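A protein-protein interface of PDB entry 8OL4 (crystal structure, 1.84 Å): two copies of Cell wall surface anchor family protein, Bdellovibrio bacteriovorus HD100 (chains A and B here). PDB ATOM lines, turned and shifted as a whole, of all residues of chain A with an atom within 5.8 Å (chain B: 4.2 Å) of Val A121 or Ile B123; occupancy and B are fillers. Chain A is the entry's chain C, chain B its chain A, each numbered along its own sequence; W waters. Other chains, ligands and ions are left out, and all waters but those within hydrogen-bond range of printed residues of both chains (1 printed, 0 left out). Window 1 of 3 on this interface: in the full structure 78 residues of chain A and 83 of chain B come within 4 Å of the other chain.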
ATOM      1  N   MET A 113     -27.064  19.568 -27.634  1.00  0.00           N
ATOM      2  CA  MET A 113     -27.399  18.181 -27.360  1.00  0.00           C
ATOM      3  C   MET A 113     -27.194  17.351 -28.621  1.00  0.00           C
ATOM      4  O   MET A 113     -27.496  17.808 -29.724  1.00  0.00           O
ATOM      5  CB  MET A 113     -28.842  18.044 -26.877  1.00  0.00           C
ATOM      6  CG  MET A 113     -29.200  16.657 -26.417  1.00  0.00           C
ATOM      7  SD  MET A 113     -30.884  16.569 -25.785  1.00  0.00           S
ATOM      8  CE  MET A 113     -30.854  17.864 -24.571  1.00  0.00           C
ATOM      9  N   ARG A 114     -26.694  16.133 -28.446  1.00  0.00           N
ATOM     10  CA  ARG A 114     -26.483  15.216 -29.554  1.00  0.00           C
ATOM     11  C   ARG A 114     -27.033  13.843 -29.192  1.00  0.00           C
ATOM     12  O   ARG A 114     -26.849  13.363 -28.071  1.00  0.00           O
ATOM     13  CB  ARG A 114     -24.987  15.112 -29.897  1.00  0.00           C
ATOM     14  CG  ARG A 114     -24.697  14.199 -31.042  1.00  0.00           C
ATOM     15  CD  ARG A 114     -23.243  14.222 -31.387  1.00  0.00           C
ATOM     16  NE  ARG A 114     -22.821  15.483 -31.982  1.00  0.00           N
ATOM     17  CZ  ARG A 114     -21.761  15.587 -32.777  1.00  0.00           C
ATOM     18  NH1 ARG A 114     -21.064  14.495 -33.068  1.00  0.00           N
ATOM     19  NH2 ARG A 114     -21.404  16.761 -33.286  1.00  0.00           N
ATOM     20  N   ILE A 115     -27.720  13.211 -30.137  1.00  0.00           N
ATOM     21  CA  ILE A 115     -28.167  11.832 -29.998  1.00  0.00           C
ATOM     22  C   ILE A 115     -27.440  11.017 -31.062  1.00  0.00           C
ATOM     23  O   ILE A 115     -27.603  11.276 -32.263  1.00  0.00           O
ATOM     24  CB  ILE A 115     -29.694  11.711 -30.140  1.00  0.00           C
ATOM     25  CG1 ILE A 115     -30.404  12.668 -29.164  1.00  0.00           C
ATOM     26  CG2 ILE A 115     -30.119  10.248 -29.965  1.00  0.00           C
ATOM     27  CD1 ILE A 115     -31.939  12.764 -29.364  1.00  0.00           C
ATOM     28  N   SER A 116     -26.623  10.059 -30.628  1.00  0.00           N
ATOM     29  CA  SER A 116     -25.809   9.281 -31.553  1.00  0.00           C
ATOM     30  C   SER A 116     -26.589   8.105 -32.145  1.00  0.00           C
ATOM     31  O   SER A 116     -27.684   7.762 -31.702  1.00  0.00           O
ATOM     32  CB  SER A 116     -24.561   8.760 -30.856  1.00  0.00           C
ATOM     33  OG  SER A 116     -23.587   9.775 -30.808  1.00  0.00           O
ATOM     34  N   GLY A 119     -28.032   5.636 -30.025  1.00  0.00           N
ATOM     35  CA  GLY A 119     -29.003   6.113 -29.068  1.00  0.00           C
ATOM     36  C   GLY A 119     -28.419   6.846 -27.883  1.00  0.00           C
ATOM     37  O   GLY A 119     -29.187   7.376 -27.069  1.00  0.00           O
ATOM     38  N   ASN A 120     -27.095   6.904 -27.759  1.00  0.00           N
ATOM     39  CA  ASN A 120     -26.485   7.600 -26.632  1.00  0.00           C
ATOM     40  C   ASN A 120     -26.611   9.110 -26.798  1.00  0.00           C
ATOM     41  O   ASN A 120     -26.425   9.653 -27.894  1.00  0.00           O
ATOM     42  CB  ASN A 120     -25.011   7.221 -26.490  1.00  0.00           C
ATOM     43  CG  ASN A 120     -24.821   5.750 -26.151  1.00  0.00           C
ATOM     44  OD1 ASN A 120     -25.792   5.011 -25.973  1.00  0.00           O
ATOM     45  ND2 ASN A 120     -23.560   5.313 -26.071  1.00  0.00           N
ATOM     46  N   VAL A 121     -26.884   9.790 -25.685  1.00  0.00           N
ATOM     47  CA  VAL A 121     -27.173  11.221 -25.663  1.00  0.00           C
ATOM     48  C   VAL A 121     -26.058  11.949 -24.922  1.00  0.00           C
ATOM     49  O   VAL A 121     -25.617  11.509 -23.850  1.00  0.00           O
ATOM     50  CB  VAL A 121     -28.543  11.489 -25.017  1.00  0.00           C
ATOM     51  CG1 VAL A 121     -28.749  12.984 -24.741  1.00  0.00           C
ATOM     52  CG2 VAL A 121     -29.629  10.927 -25.899  1.00  0.00           C
ATOM     53  N   GLY A 122     -25.587  13.043 -25.514  1.00  0.00           N
ATOM     54  CA  GLY A 122     -24.669  13.952 -24.865  1.00  0.00           C
ATOM     55  C   GLY A 122     -25.257  15.344 -24.719  1.00  0.00           C
ATOM     56  O   GLY A 122     -25.818  15.902 -25.671  1.00  0.00           O
ATOM     57  N   ILE A 123     -25.155  15.910 -23.521  1.00  0.00           N
ATOM     58  CA  ILE A 123     -25.594  17.272 -23.242  1.00  0.00           C
ATOM     59  C   ILE A 123     -24.356  18.063 -22.857  1.00  0.00           C
ATOM     60  O   ILE A 123     -23.756  17.816 -21.799  1.00  0.00           O
ATOM     61  CB  ILE A 123     -26.649  17.330 -22.131  1.00  0.00           C
ATOM     62  CG1 ILE A 123     -27.848  16.454 -22.499  1.00  0.00           C
ATOM     63  CG2 ILE A 123     -27.059  18.793 -21.875  1.00  0.00           C
ATOM     64  CD1 ILE A 123     -28.903  16.377 -21.395  1.00  0.00           C
ATOM     65  N   THR A 127     -19.214  13.646 -26.889  1.00  0.00           N
ATOM     66  CA  THR A 127     -18.733  12.311 -26.541  1.00  0.00           C
ATOM     67  C   THR A 127     -19.884  11.528 -25.919  1.00  0.00           C
ATOM     68  O   THR A 127     -20.263  11.778 -24.774  1.00  0.00           O
ATOM     69  CB  THR A 127     -17.549  12.388 -25.578  1.00  0.00           C
ATOM     70  OG1 THR A 127     -17.947  13.072 -24.386  1.00  0.00           O
ATOM     71  CG2 THR A 127     -16.391  13.140 -26.213  1.00  0.00           C
ATOM     72  N   THR A 128     -20.425  10.563 -26.665  1.00  0.00           N
ATOM     73  CA  THR A 128     -21.627   9.854 -26.256  1.00  0.00           C
ATOM     74  C   THR A 128     -21.291   8.417 -25.863  1.00  0.00           C
ATOM     75  O   THR A 128     -21.813   7.455 -26.442  1.00  0.00           O
ATOM     76  CB  THR A 128     -22.663   9.891 -27.383  1.00  0.00           C
ATOM     77  OG1 THR A 128     -22.099   9.292 -28.557  1.00  0.00           O
ATOM     78  CG2 THR A 128     -23.047  11.345 -27.716  1.00  0.00           C
ATOM     79  N   GLU A 130     -21.709   6.782 -22.816  1.00  0.00           N
ATOM     80  CA  GLU A 130     -22.780   6.116 -22.102  1.00  0.00           C
ATOM     81  C   GLU A 130     -24.119   6.588 -22.656  1.00  0.00           C
ATOM     82  O   GLU A 130     -24.192   7.477 -23.508  1.00  0.00           O
ATOM     83  CB  GLU A 130     -22.672   6.369 -20.595  1.00  0.00           C
ATOM     84  CG  GLU A 130     -21.302   6.040 -20.002  1.00  0.00           C
ATOM     85  CD  GLU A 130     -20.966   4.552 -20.061  1.00  0.00           C
ATOM     86  OE1 GLU A 130     -21.891   3.739 -20.276  1.00  0.00           O
ATOM     87  OE2 GLU A 130     -19.772   4.192 -19.896  1.00  0.00           O
ATOM     88  N   LYS A 131     -25.194   5.982 -22.155  1.00  0.00           N
ATOM     89  CA  LYS A 131     -26.523   6.292 -22.670  1.00  0.00           C
ATOM     90  C   LYS A 131     -26.851   7.767 -22.473  1.00  0.00           C
ATOM     91  O   LYS A 131     -27.507   8.385 -23.322  1.00  0.00           O
ATOM     92  CB  LYS A 131     -27.562   5.387 -21.996  1.00  0.00           C
ATOM     93  CG  LYS A 131     -28.947   5.362 -22.674  1.00  0.00           C
ATOM     94  CD  LYS A 131     -28.869   5.000 -24.149  1.00  0.00           C
ATOM     95  CE  LYS A 131     -28.414   3.554 -24.374  1.00  0.00           C
ATOM     96  NZ  LYS A 131     -28.316   3.258 -25.839  1.00  0.00           N
ATOM     97  N   LEU A 132     -26.400   8.349 -21.361  1.00  0.00           N
ATOM     98  CA  LEU A 132     -26.522   9.780 -21.114  1.00  0.00           C
ATOM     99  C   LEU A 132     -25.198  10.277 -20.552  1.00  0.00           C
ATOM    100  O   LEU A 132     -24.621   9.653 -19.653  1.00  0.00           O
ATOM    101  CB  LEU A 132     -27.693  10.104 -20.162  1.00  0.00           C
ATOM    102  CG  LEU A 132     -27.850  11.581 -19.771  1.00  0.00           C
ATOM    103  CD1 LEU A 132     -28.126  12.480 -20.982  1.00  0.00           C
ATOM    104  CD2 LEU A 132     -28.917  11.783 -18.673  1.00  0.00           C
ATOM    105  N   ASN A 133     -24.716  11.383 -21.118  1.00  0.00           N
ATOM    106  CA  ASN A 133     -23.431  11.988 -20.795  1.00  0.00           C
ATOM    107  C   ASN A 133     -23.672  13.479 -20.621  1.00  0.00           C
ATOM    108  O   ASN A 133     -24.112  14.141 -21.565  1.00  0.00           O
ATOM    109  CB  ASN A 133     -22.394  11.756 -21.908  1.00  0.00           C
ATOM    110  CG  ASN A 133     -22.350  10.314 -22.386  1.00  0.00           C
ATOM    111  OD1 ASN A 133     -21.514   9.522 -21.944  1.00  0.00           O
ATOM    112  ND2 ASN A 133     -23.242   9.970 -23.294  1.00  0.00           N
ATOM    113  N   VAL A 134     -23.383  14.006 -19.436  1.00  0.00           N
ATOM    114  CA  VAL A 134     -23.592  15.419 -19.147  1.00  0.00           C
ATOM    115  C   VAL A 134     -22.244  16.039 -18.817  1.00  0.00           C
ATOM    116  O   VAL A 134     -21.540  15.566 -17.915  1.00  0.00           O
ATOM    117  CB  VAL A 134     -24.586  15.636 -17.994  1.00  0.00           C
ATOM    118  CG1 VAL A 134     -24.753  17.135 -17.753  1.00  0.00           C
ATOM    119  CG2 VAL A 134     -25.948  14.978 -18.318  1.00  0.00           C
ATOM    120  N   ALA B 112     -34.584   6.686 -30.124  1.00  0.00           N
ATOM    121  CA  ALA B 112     -33.623   6.901 -29.056  1.00  0.00           C
ATOM    122  C   ALA B 112     -34.174   7.702 -27.898  1.00  0.00           C
ATOM    123  O   ALA B 112     -33.726   7.502 -26.771  1.00  0.00           O
ATOM    124  CB  ALA B 112     -32.376   7.614 -29.585  1.00  0.00           C
ATOM    125  N   MET B 113     -35.139   8.592 -28.130  1.00  0.00           N
ATOM    126  CA  MET B 113     -35.671   9.394 -27.033  1.00  0.00           C
ATOM    127  C   MET B 113     -37.169   9.611 -27.211  1.00  0.00           C
ATOM    128  O   MET B 113     -37.634   9.900 -28.312  1.00  0.00           O
ATOM    129  CB  MET B 113     -34.951  10.753 -26.924  1.00  0.00           C
ATOM    130  CG  MET B 113     -35.273  11.533 -25.644  1.00  0.00           C
ATOM    131  SD  MET B 113     -34.110  12.884 -25.288  1.00  0.00           S
ATOM    132  CE  MET B 113     -34.509  14.041 -26.602  1.00  0.00           C
ATOM    133  N   GLY B 122     -37.863   9.529 -21.774  1.00  0.00           N
ATOM    134  CA  GLY B 122     -37.176   8.260 -21.747  1.00  0.00           C
ATOM    135  C   GLY B 122     -36.054   8.245 -22.760  1.00  0.00           C
ATOM    136  O   GLY B 122     -36.253   8.574 -23.929  1.00  0.00           O
ATOM    137  N   ILE B 123     -34.869   7.846 -22.331  1.00  0.00           N
ATOM    138  CA  ILE B 123     -33.724   7.688 -23.214  1.00  0.00           C
ATOM    139  C   ILE B 123     -33.401   6.204 -23.257  1.00  0.00           C
ATOM    140  O   ILE B 123     -32.900   5.631 -22.277  1.00  0.00           O
ATOM    141  CB  ILE B 123     -32.521   8.519 -22.748  1.00  0.00           C
ATOM    142  CG1 ILE B 123     -32.909  10.003 -22.676  1.00  0.00           C
ATOM    143  CG2 ILE B 123     -31.322   8.310 -23.697  1.00  0.00           C
ATOM    144  CD1 ILE B 123     -31.749  10.942 -22.289  1.00  0.00           C
ATOM    145  N   GLY B 124     -33.709   5.579 -24.386  1.00  0.00           N
ATOM    146  CA  GLY B 124     -33.547   4.161 -24.542  1.00  0.00           C
ATOM    147  C   GLY B 124     -34.672   3.333 -23.975  1.00  0.00           C
ATOM    148  O   GLY B 124     -34.563   2.103 -23.980  1.00  0.00           O
ATOM    149  N   THR B 125     -35.728   3.967 -23.459  1.00  0.00           N
ATOM    150  CA  THR B 125     -36.928   3.271 -23.017  1.00  0.00           C
ATOM    151  C   THR B 125     -38.153   4.106 -23.366  1.00  0.00           C
ATOM    152  O   THR B 125     -38.110   5.340 -23.373  1.00  0.00           O
ATOM    153  CB  THR B 125     -36.923   2.986 -21.504  1.00  0.00           C
ATOM    154  OG1 THR B 125     -38.135   2.307 -21.136  1.00  0.00           O
ATOM    155  CG2 THR B 125     -36.829   4.268 -20.733  1.00  0.00           C
ATOM    156  N   ASN B 133     -35.954   8.961 -17.428  1.00  0.00           N
ATOM    157  CA  ASN B 133     -35.663   7.544 -17.332  1.00  0.00           C
ATOM    158  C   ASN B 133     -34.562   7.234 -18.322  1.00  0.00           C
ATOM    159  O   ASN B 133     -34.655   7.625 -19.491  1.00  0.00           O
ATOM    160  CB  ASN B 133     -36.898   6.709 -17.649  1.00  0.00           C
ATOM    161  CG  ASN B 133     -38.128   7.250 -16.996  1.00  0.00           C
ATOM    162  OD1 ASN B 133     -38.531   6.782 -15.923  1.00  0.00           O
ATOM    163  ND2 ASN B 133     -38.741   8.251 -17.621  1.00  0.00           N
ATOM    164  N   VAL B 134     -33.525   6.546 -17.868  1.00  0.00           N
ATOM    165  CA  VAL B 134     -32.391   6.228 -18.729  1.00  0.00           C
ATOM    166  C   VAL B 134     -32.153   4.729 -18.684  1.00  0.00           C
ATOM    167  O   VAL B 134     -31.910   4.165 -17.608  1.00  0.00           O
ATOM    168  CB  VAL B 134     -31.124   6.992 -18.318  1.00  0.00           C
ATOM    169  CG1 VAL B 134     -29.940   6.566 -19.186  1.00  0.00           C
ATOM    170  CG2 VAL B 134     -31.372   8.483 -18.422  1.00  0.00           C
ATOM    171  N   GLN B 135     -32.233   4.086 -19.846  1.00  0.00           N
ATOM    172  CA  GLN B 135     -31.968   2.656 -19.963  1.00  0.00           C
ATOM    173  C   GLN B 135     -30.489   2.478 -20.313  1.00  0.00           C
ATOM    174  O   GLN B 135     -30.099   2.307 -21.470  1.00  0.00           O
ATOM    175  CB  GLN B 135     -32.884   2.033 -21.008  1.00  0.00           C
ATOM    176  CG  GLN B 135     -32.869   0.514 -21.036  1.00  0.00           C
ATOM    177  CD  GLN B 135     -33.420  -0.096 -19.758  1.00  0.00           C
ATOM    178  OE1 GLN B 135     -34.277   0.487 -19.098  1.00  0.00           O
ATOM    179  NE2 GLN B 135     -32.932  -1.272 -19.409  1.00  0.00           N
HETATM  180  O   HOH W   1     -31.326   5.999 -26.502  1.00  0.00           O
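Among the printed residues, merely in contact across the chains: Lys A131 with Gln B135 (3.5 Å), Ile A115 with Ala B112 (3.5 Å), Gly A119 with Ala B112 (3.7 Å), Val A121 with Ile B123 (3.8 Å), Lys A131 with Val B134 (3.8 Å), Lys A131 with Ile B123 (3.8 Å) and Ile A115 with Met B113 (3.98 Å).
Of the printed residues of chain B, Val A121 touches Ile B123. Ile B123 touches two residues of chain A. Printed residues of chain A within 4 Å of Val B134: Lys A131 (3.8 Å). Of the printed residues of chain B, Gly A119 touches Ala B112 (3.7 Å). Of the printed residues of chain A, Gln B135 touches Lys A131 (3.5 Å). Of the printed residues of chain B, Ile A115 touches Ala B112 (3.5 Å) and Met B113 (3.98 Å). Gly A122 touches none of the printed residues of chain B. The nearest printed residue of chain B that does not touch Val A121 is Met B113 (4.9 Å).
The backbone carbonyl oxygen (O) of Lys A131 is in hydrogen-bond range of the backbone NH (N) of Val A121, 2.8 Å away. The backbone NH of Ile B123 is in hydrogen-bond range of the backbone carbonyl oxygen of Asn B133 (2.9 Å). N of Gln B135 is in hydrogen-bond range of O of Ile B123 (3.0 Å). N of Asn A133 lies within hydrogen-bond range of O of Val A121, 2.9 Å away. OD1 of Asn A120 sits at hydrogen-bond distance from NZ of Lys A131 (3.1 Å). O of Ala B112 is in hydrogen-bond range of N of Gly B124, at 3.1 Å.
Positions printed for both chains: 113, 122, 123, 133 and 134. Of the 7 pairs that touch across the chains among the printed residues, none has its exchanged pair printed and touching as well.
Water W1 lies within hydrogen-bond range of O of Gly A119 (2.6 Å), O of Ala B112 (2.8 Å) and N of Gly B124 (3.2 Å).
Of the 16 printed residues of chain A, 4 touch a printed residue of chain B. Printed residues of chain A that touch a printed residue of chain B: Ile A115, Gly A119, Val A121 and Lys A131. Of the 9 printed residues of chain B, 5 touch a printed residue of chain A.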
